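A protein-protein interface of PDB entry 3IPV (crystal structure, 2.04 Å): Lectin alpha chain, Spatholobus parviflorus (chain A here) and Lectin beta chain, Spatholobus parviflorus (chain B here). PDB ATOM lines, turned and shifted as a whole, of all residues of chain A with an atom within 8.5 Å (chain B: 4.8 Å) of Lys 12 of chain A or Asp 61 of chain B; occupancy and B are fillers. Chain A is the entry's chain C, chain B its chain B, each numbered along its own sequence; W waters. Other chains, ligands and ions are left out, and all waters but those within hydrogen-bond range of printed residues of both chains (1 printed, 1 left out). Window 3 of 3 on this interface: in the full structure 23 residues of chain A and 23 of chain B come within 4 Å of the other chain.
The side-chain carboxylate of Asp 61 of chain B lies within salt-bridge range of the side-chain amino group of Lys 12 of chain A (2.8 Å).
The side-chain amino group (NZ) of Lys 12 of chain A sits close to the side-chain amide nitrogen (ND2) of Asn 58 of chain B (2.7 Å).
The side-chain carboxylate (OE2) of Glu 2 of chain B is in hydrogen-bond range of the backbone NH (N) of Ser 9 of chain A (3.0 Å).
OE2 of Glu 2 of chain B lies within hydrogen-bond range of N of Lys 10 of chain A, 3.3 Å away.
The backbone NH (N) of Leu 237 of chain B is in hydrogen-bond range of the backbone carbonyl oxygen (O) of Glu 2 of chain B, at 2.9 Å.
The backbone carbonyl oxygen (O) of Leu 66 of chain B is in hydrogen-bond range of the backbone NH (N) of Asp 61 of chain B, 2.9 Å away.
The backbone NH (N) of Lys 12 of chain A is in hydrogen-bond range of the side-chain carboxylate (OE1) of Glu 15 of chain A, at 2.7 Å.
The side-chain hydroxyl (OG1) of Thr 64 of chain B sits at hydrogen-bond distance from the side-chain carboxylate (OD2) of Asp 61 of chain B (2.7 Å).
OD1 of Asn 58 of chain B sits close to O of Trp 60 of chain B (3.3 Å).
The side-chain amide oxygen (OD1) of Asn 58 of chain B sits close to the backbone carbonyl oxygen (O) of Glu 206 of chain B.
Among the printed residues, pairs that only touch across the chains: Phe 8 of chain A with Glu 2 of chain B and Lys 12 of chain A with Leu 237 of chain B.
Of the printed residues of chain B, Phe 8 of chain A touches Glu 2 (3.8 Å).
Of the printed residues of chain B, Ser 9 of chain A touches Glu 2.
Lys 12 of chain A touches just these residues of chain B: Asn 58, Asp 61 and Leu 237.
Of the printed residues of chain A, Glu 2 of chain B touches Phe 8 (3.8 Å), Ser 9 (3.0 Å) and Lys 10 (2.9 Å).
Printed residues of chain A within 4 Å of Asn 58 of chain B: Lys 12 (2.7 Å).
Of chain A, only Lys 12 comes within 4 Å of Asp 61 of chain B.
Ala 63 of chain B touches none of the printed residues of chain A.
Glu 206 of chain B touches none of the printed residues of chain A.
Printed residues of chain A within 4 Å of Leu 237 of chain B: Lys 12 (3.97 Å).
The nearest residue of chain B that does not touch Lys 12 of chain A is Glu 2 of chain B (4.1 Å).
The nearest residue of chain A that does not touch Asp 61 of chain B is Lys 10 of chain A (6.1 Å).
The nearest printed residue of chain B that does not touch Lys 10 of chain A is Asp 61 of chain B (6.1 Å).
Printed residues of chain A that touch a printed residue of chain B: Phe 8, Ser 9, Lys 10 and Lys 12.
Hydrophobic or aromatic side chains of chain B within 4 Å of the printed part of chain A: Leu 237.
Among the printed residues, 6 pairs touch across the chains.
Water W1 lies within hydrogen-bond range of the side-chain carboxylate (OE1) of Glu 2 of chain B (2.9 Å), the side-chain amide nitrogen (ND2) of Asn 58 of chain B (3.0 Å) and the side-chain carboxylate (OE2) of Glu 15 of chain A (3.1 Å).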
ATOM      1  N   PHE A   8       0.981   5.432  19.798  1.00  0.00           N
ATOM      2  CA  PHE A   8      -0.431   5.789  19.733  1.00  0.00           C
ATOM      3  C   PHE A   8      -1.201   4.486  19.668  1.00  0.00           C
ATOM      4  O   PHE A   8      -1.319   3.887  18.568  1.00  0.00           O
ATOM      5  CB  PHE A   8      -0.758   6.585  18.445  1.00  0.00           C
ATOM      6  CG  PHE A   8      -0.033   7.896  18.330  1.00  0.00           C
ATOM      7  CD1 PHE A   8       1.212   7.981  17.700  1.00  0.00           C
ATOM      8  CD2 PHE A   8      -0.623   9.069  18.751  1.00  0.00           C
ATOM      9  CE1 PHE A   8       1.888   9.178  17.542  1.00  0.00           C
ATOM     10  CE2 PHE A   8       0.050  10.307  18.604  1.00  0.00           C
ATOM     11  CZ  PHE A   8       1.323  10.346  17.968  1.00  0.00           C
ATOM     12  N   SER A   9      -1.710   4.010  20.794  1.00  0.00           N
ATOM     13  CA  SER A   9      -2.567   2.845  20.711  1.00  0.00           C
ATOM     14  C   SER A   9      -4.000   3.179  20.305  1.00  0.00           C
ATOM     15  O   SER A   9      -4.743   2.304  19.902  1.00  0.00           O
ATOM     16  CB  SER A   9      -2.449   1.929  21.912  1.00  0.00           C
ATOM     17  OG  SER A   9      -1.166   1.218  21.806  1.00  0.00           O
ATOM     18  N   LYS A  10      -4.368   4.449  20.403  1.00  0.00           N
ATOM     19  CA  LYS A  10      -5.396   5.034  19.515  1.00  0.00           C
ATOM     20  C   LYS A  10      -5.049   6.457  19.364  1.00  0.00           C
ATOM     21  O   LYS A  10      -4.086   6.910  19.972  1.00  0.00           O
ATOM     22  CB  LYS A  10      -6.778   4.954  20.145  1.00  0.00           C
ATOM     23  CG  LYS A  10      -6.739   5.473  21.560  1.00  0.00           C
ATOM     24  CD  LYS A  10      -7.723   4.624  22.383  1.00  0.00           C
ATOM     25  CE  LYS A  10      -8.012   5.371  23.622  1.00  0.00           C
ATOM     26  NZ  LYS A  10      -8.513   6.721  23.201  1.00  0.00           N
ATOM     27  N   PHE A  11      -5.860   7.201  18.608  1.00  0.00           N
ATOM     28  CA  PHE A  11      -5.647   8.622  18.394  1.00  0.00           C
ATOM     29  C   PHE A  11      -6.788   9.399  19.088  1.00  0.00           C
ATOM     30  O   PHE A  11      -7.790   8.791  19.508  1.00  0.00           O
ATOM     31  CB  PHE A  11      -5.587   8.918  16.858  1.00  0.00           C
ATOM     32  CG  PHE A  11      -4.431   8.164  16.128  1.00  0.00           C
ATOM     33  CD1 PHE A  11      -3.108   8.648  16.132  1.00  0.00           C
ATOM     34  CD2 PHE A  11      -4.686   6.981  15.458  1.00  0.00           C
ATOM     35  CE1 PHE A  11      -2.059   7.950  15.471  1.00  0.00           C
ATOM     36  CE2 PHE A  11      -3.644   6.274  14.789  1.00  0.00           C
ATOM     37  CZ  PHE A  11      -2.343   6.733  14.801  1.00  0.00           C
ATOM     38  N   LYS A  12      -6.640  10.709  19.244  1.00  0.00           N
ATOM     39  CA  LYS A  12      -7.673  11.474  19.969  1.00  0.00           C
ATOM     40  C   LYS A  12      -8.006  12.702  19.188  1.00  0.00           C
ATOM     41  O   LYS A  12      -7.166  13.159  18.432  1.00  0.00           O
ATOM     42  CB  LYS A  12      -7.181  11.894  21.358  1.00  0.00           C
ATOM     43  CG  LYS A  12      -7.127  10.764  22.435  1.00  0.00           C
ATOM     44  CD  LYS A  12      -6.031  11.069  23.487  1.00  0.00           C
ATOM     45  CE  LYS A  12      -5.829   9.991  24.567  1.00  0.00           C
ATOM     46  NZ  LYS A  12      -5.431  10.639  25.847  1.00  0.00           N
ATOM     47  N   PRO A  13      -9.214  13.287  19.406  1.00  0.00           N
ATOM     48  CA  PRO A  13      -9.549  14.518  18.676  1.00  0.00           C
ATOM     49  C   PRO A  13      -8.571  15.687  18.968  1.00  0.00           C
ATOM     50  O   PRO A  13      -8.201  16.438  18.040  1.00  0.00           O
ATOM     51  CB  PRO A  13     -11.001  14.842  19.150  1.00  0.00           C
ATOM     52  CG  PRO A  13     -11.572  13.485  19.541  1.00  0.00           C
ATOM     53  CD  PRO A  13     -10.385  12.701  20.094  1.00  0.00           C
ATOM     54  N   LEU A  14      -8.162  15.873  20.227  1.00  0.00           N
ATOM     55  CA  LEU A  14      -7.081  16.780  20.448  1.00  0.00           C
ATOM     56  C   LEU A  14      -5.750  15.971  20.461  1.00  0.00           C
ATOM     57  O   LEU A  14      -5.477  15.249  21.450  1.00  0.00           O
ATOM     58  CB  LEU A  14      -7.291  17.625  21.726  1.00  0.00           C
ATOM     59  CG  LEU A  14      -6.004  18.322  22.199  1.00  0.00           C
ATOM     60  CD1 LEU A  14      -5.540  19.314  21.151  1.00  0.00           C
ATOM     61  CD2 LEU A  14      -6.192  18.977  23.545  1.00  0.00           C
ATOM     62  N   GLU A  15      -4.950  16.057  19.388  1.00  0.00           N
ATOM     63  CA  GLU A  15      -3.682  15.303  19.314  1.00  0.00           C
ATOM     64  C   GLU A  15      -2.524  16.254  18.923  1.00  0.00           C
ATOM     65  O   GLU A  15      -2.146  16.266  17.756  1.00  0.00           O
ATOM     66  CB  GLU A  15      -3.848  14.190  18.241  1.00  0.00           C
ATOM     67  CG  GLU A  15      -2.877  13.033  18.287  1.00  0.00           C
ATOM     68  CD  GLU A  15      -3.077  12.148  19.513  1.00  0.00           C
ATOM     69  OE1 GLU A  15      -4.073  11.398  19.600  1.00  0.00           O
ATOM     70  OE2 GLU A  15      -2.223  12.246  20.421  1.00  0.00           O
ATOM     71  N   PRO A  16      -2.002  17.086  19.857  1.00  0.00           N
ATOM     72  CA  PRO A  16      -0.976  18.057  19.369  1.00  0.00           C
ATOM     73  C   PRO A  16       0.377  17.481  19.069  1.00  0.00           C
ATOM     74  O   PRO A  16       1.143  18.176  18.447  1.00  0.00           O
ATOM     75  CB  PRO A  16      -0.854  19.118  20.495  1.00  0.00           C
ATOM     76  CG  PRO A  16      -1.414  18.482  21.689  1.00  0.00           C
ATOM     77  CD  PRO A  16      -2.470  17.442  21.210  1.00  0.00           C
ATOM     78  N   ASN A  17       0.663  16.224  19.432  1.00  0.00           N
ATOM     79  CA  ASN A  17       1.904  15.570  18.954  1.00  0.00           C
ATOM     80  C   ASN A  17       1.775  14.901  17.560  1.00  0.00           C
ATOM     81  O   ASN A  17       2.694  14.198  17.124  1.00  0.00           O
ATOM     82  CB  ASN A  17       2.403  14.548  19.990  1.00  0.00           C
ATOM     83  CG  ASN A  17       1.374  13.452  20.299  1.00  0.00           C
ATOM     84  OD1 ASN A  17       0.201  13.506  19.846  1.00  0.00           O
ATOM     85  ND2 ASN A  17       1.808  12.432  21.088  1.00  0.00           N
ATOM     86  N   LEU A  18       0.621  15.072  16.894  1.00  0.00           N
ATOM     87  CA  LEU A  18       0.484  14.719  15.492  1.00  0.00           C
ATOM     88  C   LEU A  18       0.323  16.023  14.656  1.00  0.00           C
ATOM     89  O   LEU A  18      -0.360  16.984  15.077  1.00  0.00           O
ATOM     90  CB  LEU A  18      -0.760  13.883  15.255  1.00  0.00           C
ATOM     91  CG  LEU A  18      -0.817  12.375  15.020  1.00  0.00           C
ATOM     92  CD1 LEU A  18      -2.236  11.916  14.544  1.00  0.00           C
ATOM     93  CD2 LEU A  18       0.244  11.932  14.066  1.00  0.00           C
ATOM     94  N   LEU A  20      -1.535  17.012  11.414  1.00  0.00           N
ATOM     95  CA  LEU A  20      -2.509  16.675  10.344  1.00  0.00           C
ATOM     96  C   LEU A  20      -2.419  17.598   9.152  1.00  0.00           C
ATOM     97  O   LEU A  20      -2.501  18.821   9.298  1.00  0.00           O
ATOM     98  CB  LEU A  20      -3.955  16.600  10.917  1.00  0.00           C
ATOM     99  CG  LEU A  20      -4.047  15.705  12.181  1.00  0.00           C
ATOM    100  CD1 LEU A  20      -5.370  15.856  13.017  1.00  0.00           C
ATOM    101  CD2 LEU A  20      -3.812  14.284  11.748  1.00  0.00           C
ATOM    102  N   LEU A  25      -8.123  13.666   9.603  1.00  0.00           N
ATOM    103  CA  LEU A  25      -8.762  14.017  10.838  1.00  0.00           C
ATOM    104  C   LEU A  25      -8.805  12.781  11.768  1.00  0.00           C
ATOM    105  O   LEU A  25      -8.813  11.639  11.311  1.00  0.00           O
ATOM    106  CB  LEU A  25     -10.184  14.560  10.587  1.00  0.00           C
ATOM    107  CG  LEU A  25     -11.383  13.715  10.128  1.00  0.00           C
ATOM    108  CD1 LEU A  25     -11.918  12.811  11.193  1.00  0.00           C
ATOM    109  CD2 LEU A  25     -12.548  14.557   9.651  1.00  0.00           C
ATOM    110  N   VAL A  26      -8.912  13.002  13.061  1.00  0.00           N
ATOM    111  CA  VAL A  26      -9.115  11.881  13.929  1.00  0.00           C
ATOM    112  C   VAL A  26     -10.594  11.991  14.385  1.00  0.00           C
ATOM    113  O   VAL A  26     -11.104  13.097  14.590  1.00  0.00           O
ATOM    114  CB  VAL A  26      -8.105  11.919  15.093  1.00  0.00           C
ATOM    115  CG1 VAL A  26      -8.428  10.936  16.121  1.00  0.00           C
ATOM    116  CG2 VAL A  26      -6.679  11.749  14.580  1.00  0.00           C
ATOM    117  N   THR A  27     -11.288  10.869  14.472  1.00  0.00           N
ATOM    118  CA  THR A  27     -12.733  10.857  14.846  1.00  0.00           C
ATOM    119  C   THR A  27     -12.866  10.710  16.348  1.00  0.00           C
ATOM    120  O   THR A  27     -11.902  10.276  17.044  1.00  0.00           O
ATOM    121  CB  THR A  27     -13.454   9.612  14.288  1.00  0.00           C
ATOM    122  OG1 THR A  27     -12.767   8.431  14.758  1.00  0.00           O
ATOM    123  CG2 THR A  27     -13.433   9.576  12.809  1.00  0.00           C
ATOM    124  N   VAL A  28     -14.093  10.900  16.828  1.00  0.00           N
ATOM    125  CA  VAL A  28     -14.364  10.793  18.270  1.00  0.00           C
ATOM    126  C   VAL A  28     -14.065   9.358  18.739  1.00  0.00           C
ATOM    127  O   VAL A  28     -13.609   9.168  19.861  1.00  0.00           O
ATOM    128  CB  VAL A  28     -15.842  11.146  18.640  1.00  0.00           C
ATOM    129  CG1 VAL A  28     -16.257  12.458  18.071  1.00  0.00           C
ATOM    130  CG2 VAL A  28     -16.689  10.138  18.055  1.00  0.00           C
ATOM    131  N   ALA A  29     -14.227   8.375  17.847  1.00  0.00           N
ATOM    132  CA  ALA A  29     -13.897   6.963  18.172  1.00  0.00           C
ATOM    133  C   ALA A  29     -12.371   6.640  18.159  1.00  0.00           C
ATOM    134  O   ALA A  29     -11.982   5.505  18.385  1.00  0.00           O
ATOM    135  CB  ALA A  29     -14.659   5.996  17.199  1.00  0.00           C
ATOM    136  N   GLY A  30     -11.522   7.623  17.897  1.00  0.00           N
ATOM    137  CA  GLY A  30     -10.059   7.460  17.969  1.00  0.00           C
ATOM    138  C   GLY A  30      -9.402   6.925  16.694  1.00  0.00           C
ATOM    139  O   GLY A  30      -8.258   6.443  16.708  1.00  0.00           O
ATOM    140  N   VAL A  31     -10.101   7.050  15.578  1.00  0.00           N
ATOM    141  CA  VAL A  31      -9.609   6.538  14.305  1.00  0.00           C
ATOM    142  C   VAL A  31      -8.982   7.678  13.520  1.00  0.00           C
ATOM    143  O   VAL A  31      -9.619   8.719  13.322  1.00  0.00           O
ATOM    144  CB  VAL A  31     -10.811   5.918  13.497  1.00  0.00           C
ATOM    145  CG1 VAL A  31     -10.368   5.463  12.059  1.00  0.00           C
ATOM    146  CG2 VAL A  31     -11.463   4.850  14.297  1.00  0.00           C
ATOM    147  N   LEU A  32      -7.742   7.484  13.065  1.00  0.00           N
ATOM    148  CA  LEU A  32      -7.111   8.408  12.119  1.00  0.00           C
ATOM    149  C   LEU A  32      -7.625   8.108  10.722  1.00  0.00           C
ATOM    150  O   LEU A  32      -7.219   7.140  10.113  1.00  0.00           O
ATOM    151  CB  LEU A  32      -5.572   8.362  12.190  1.00  0.00           C
ATOM    152  CG  LEU A  32      -4.717   9.092  11.167  1.00  0.00           C
ATOM    153  CD1 LEU A  32      -4.946  10.642  11.136  1.00  0.00           C
ATOM    154  CD2 LEU A  32      -3.242   8.749  11.510  1.00  0.00           C
ATOM    155  N   PHE A 229      -5.520   2.790  12.953  1.00  0.00           N
ATOM    156  CA  PHE A 229      -6.066   2.570  14.329  1.00  0.00           C
ATOM    157  C   PHE A 229      -5.039   2.734  15.417  1.00  0.00           C
ATOM    158  O   PHE A 229      -5.395   3.109  16.563  1.00  0.00           O
ATOM    159  CB  PHE A 229      -6.641   1.164  14.497  1.00  0.00           C
ATOM    160  CG  PHE A 229      -7.517   0.795  13.401  1.00  0.00           C
ATOM    161  CD1 PHE A 229      -8.599   1.577  13.129  1.00  0.00           C
ATOM    162  CD2 PHE A 229      -7.220  -0.263  12.577  1.00  0.00           C
ATOM    163  CE1 PHE A 229      -9.405   1.300  12.113  1.00  0.00           C
ATOM    164  CE2 PHE A 229      -8.041  -0.541  11.564  1.00  0.00           C
ATOM    165  CZ  PHE A 229      -9.132   0.246  11.331  1.00  0.00           C
ATOM    166  N   GLU B   2      -0.765   5.364  25.650  1.00  0.00           N
ATOM    167  CA  GLU B   2      -0.197   6.419  24.882  1.00  0.00           C
ATOM    168  C   GLU B   2       1.162   6.674  25.500  1.00  0.00           C
ATOM    169  O   GLU B   2       1.271   6.986  26.696  1.00  0.00           O
ATOM    170  CB  GLU B   2      -1.078   7.667  25.044  1.00  0.00           C
ATOM    171  CG  GLU B   2      -2.571   7.476  24.610  1.00  0.00           C
ATOM    172  CD  GLU B   2      -2.653   7.086  23.142  1.00  0.00           C
ATOM    173  OE1 GLU B   2      -2.541   7.958  22.247  1.00  0.00           O
ATOM    174  OE2 GLU B   2      -2.762   5.879  22.868  1.00  0.00           O
ATOM    175  N   ASN B  58       1.266  13.682  26.454  1.00  0.00           N
ATOM    176  CA  ASN B  58      -0.073  13.513  27.057  1.00  0.00           C
ATOM    177  C   ASN B  58       0.087  13.015  28.505  1.00  0.00           C
ATOM    178  O   ASN B  58       0.530  11.873  28.736  1.00  0.00           O
ATOM    179  CB  ASN B  58      -0.840  12.531  26.182  1.00  0.00           C
ATOM    180  CG  ASN B  58      -2.350  12.595  26.333  1.00  0.00           C
ATOM    181  OD1 ASN B  58      -2.920  13.417  27.063  1.00  0.00           O
ATOM    182  ND2 ASN B  58      -3.014  11.729  25.587  1.00  0.00           N
ATOM    183  N   TRP B  60      -2.307  13.276  31.316  1.00  0.00           N
ATOM    184  CA  TRP B  60      -3.512  12.658  31.850  1.00  0.00           C
ATOM    185  C   TRP B  60      -4.662  12.870  30.852  1.00  0.00           C
ATOM    186  O   TRP B  60      -4.509  13.620  29.907  1.00  0.00           O
ATOM    187  CB  TRP B  60      -3.847  13.183  33.264  1.00  0.00           C
ATOM    188  CG  TRP B  60      -4.348  14.652  33.352  1.00  0.00           C
ATOM    189  CD1 TRP B  60      -3.571  15.784  33.460  1.00  0.00           C
ATOM    190  CD2 TRP B  60      -5.714  15.099  33.400  1.00  0.00           C
ATOM    191  NE1 TRP B  60      -4.387  16.914  33.530  1.00  0.00           N
ATOM    192  CE2 TRP B  60      -5.698  16.515  33.507  1.00  0.00           C
ATOM    193  CE3 TRP B  60      -6.956  14.440  33.380  1.00  0.00           C
ATOM    194  CZ2 TRP B  60      -6.882  17.284  33.597  1.00  0.00           C
ATOM    195  CZ3 TRP B  60      -8.133  15.221  33.474  1.00  0.00           C
ATOM    196  CH2 TRP B  60      -8.077  16.620  33.580  1.00  0.00           C
ATOM    197  N   ASP B  61      -5.813  12.234  31.094  1.00  0.00           N
ATOM    198  CA  ASP B  61      -6.878  12.092  30.107  1.00  0.00           C
ATOM    199  C   ASP B  61      -8.249  12.298  30.783  1.00  0.00           C
ATOM    200  O   ASP B  61      -8.542  11.715  31.806  1.00  0.00           O
ATOM    201  CB  ASP B  61      -6.769  10.715  29.447  1.00  0.00           C
ATOM    202  CG  ASP B  61      -7.823  10.479  28.403  1.00  0.00           C
ATOM    203  OD1 ASP B  61      -7.756  11.121  27.343  1.00  0.00           O
ATOM    204  OD2 ASP B  61      -8.733   9.661  28.641  1.00  0.00           O
ATOM    205  N   SER B  62      -9.049  13.156  30.168  1.00  0.00           N
ATOM    206  CA  SER B  62     -10.315  13.648  30.679  1.00  0.00           C
ATOM    207  C   SER B  62     -11.390  12.544  30.647  1.00  0.00           C
ATOM    208  O   SER B  62     -12.126  12.361  31.603  1.00  0.00           O
ATOM    209  CB  SER B  62     -10.722  14.875  29.831  1.00  0.00           C
ATOM    210  OG  SER B  62     -12.069  15.242  30.049  1.00  0.00           O
ATOM    211  N   ALA B  63     -11.453  11.812  29.540  1.00  0.00           N
ATOM    212  CA  ALA B  63     -12.481  10.779  29.343  1.00  0.00           C
ATOM    213  C   ALA B  63     -12.259   9.629  30.309  1.00  0.00           C
ATOM    214  O   ALA B  63     -13.156   9.219  31.009  1.00  0.00           O
ATOM    215  CB  ALA B  63     -12.476  10.272  27.897  1.00  0.00           C
ATOM    216  N   THR B  64     -11.029   9.144  30.384  1.00  0.00           N
ATOM    217  CA  THR B  64     -10.766   8.039  31.270  1.00  0.00           C
ATOM    218  C   THR B  64     -10.511   8.480  32.733  1.00  0.00           C
ATOM    219  O   THR B  64     -10.714   7.691  33.666  1.00  0.00           O
ATOM    220  CB  THR B  64      -9.555   7.236  30.773  1.00  0.00           C
ATOM    221  OG1 THR B  64      -8.415   8.093  30.766  1.00  0.00           O
ATOM    222  CG2 THR B  64      -9.798   6.654  29.349  1.00  0.00           C
ATOM    223  N   GLY B  65     -10.017   9.702  32.933  1.00  0.00           N
ATOM    224  CA  GLY B  65      -9.563  10.121  34.282  1.00  0.00           C
ATOM    225  C   GLY B  65      -8.148   9.661  34.650  1.00  0.00           C
ATOM    226  O   GLY B  65      -7.656  10.008  35.706  1.00  0.00           O
ATOM    227  N   LEU B  66      -7.482   8.901  33.787  1.00  0.00           N
ATOM    228  CA  LEU B  66      -6.147   8.338  34.122  1.00  0.00           C
ATOM    229  C   LEU B  66      -5.003   9.340  33.942  1.00  0.00           C
ATOM    230  O   LEU B  66      -5.108  10.277  33.150  1.00  0.00           O
ATOM    231  CB  LEU B  66      -5.857   7.031  33.332  1.00  0.00           C
ATOM    232  CG  LEU B  66      -6.876   5.902  33.585  1.00  0.00           C
ATOM    233  CD1 LEU B  66      -6.696   4.830  32.586  1.00  0.00           C
ATOM    234  CD2 LEU B  66      -6.764   5.325  34.957  1.00  0.00           C
ATOM    235  N   GLU B 206      -3.976  18.458  30.447  1.00  0.00           N
ATOM    236  CA  GLU B 206      -3.801  17.125  29.855  1.00  0.00           C
ATOM    237  C   GLU B 206      -2.513  16.954  29.028  1.00  0.00           C
ATOM    238  O   GLU B 206      -1.939  15.870  28.987  1.00  0.00           O
ATOM    239  CB  GLU B 206      -5.010  16.746  29.020  1.00  0.00           C
ATOM    240  CG  GLU B 206      -6.302  16.612  29.836  1.00  0.00           C
ATOM    241  CD  GLU B 206      -7.522  16.368  28.949  1.00  0.00           C
ATOM    242  OE1 GLU B 206      -7.723  15.214  28.504  1.00  0.00           O
ATOM    243  OE2 GLU B 206      -8.292  17.328  28.685  1.00  0.00           O
ATOM    244  N   LEU B 237       0.812   6.658  29.517  1.00  0.00           N
ATOM    245  CA  LEU B 237      -0.577   6.966  29.892  1.00  0.00           C
ATOM    246  C   LEU B 237      -1.532   5.841  29.479  1.00  0.00           C
ATOM    247  O   LEU B 237      -1.871   5.682  28.289  1.00  0.00           O
ATOM    248  CB  LEU B 237      -1.015   8.298  29.260  1.00  0.00           C
ATOM    249  CG  LEU B 237      -2.465   8.786  29.454  1.00  0.00           C
ATOM    250  CD1 LEU B 237      -2.760   9.070  30.978  1.00  0.00           C
ATOM    251  CD2 LEU B 237      -2.716  10.002  28.670  1.00  0.00           C
HETATM  252  O   HOH W   1      -1.909  10.661  23.037  1.00  0.00           O
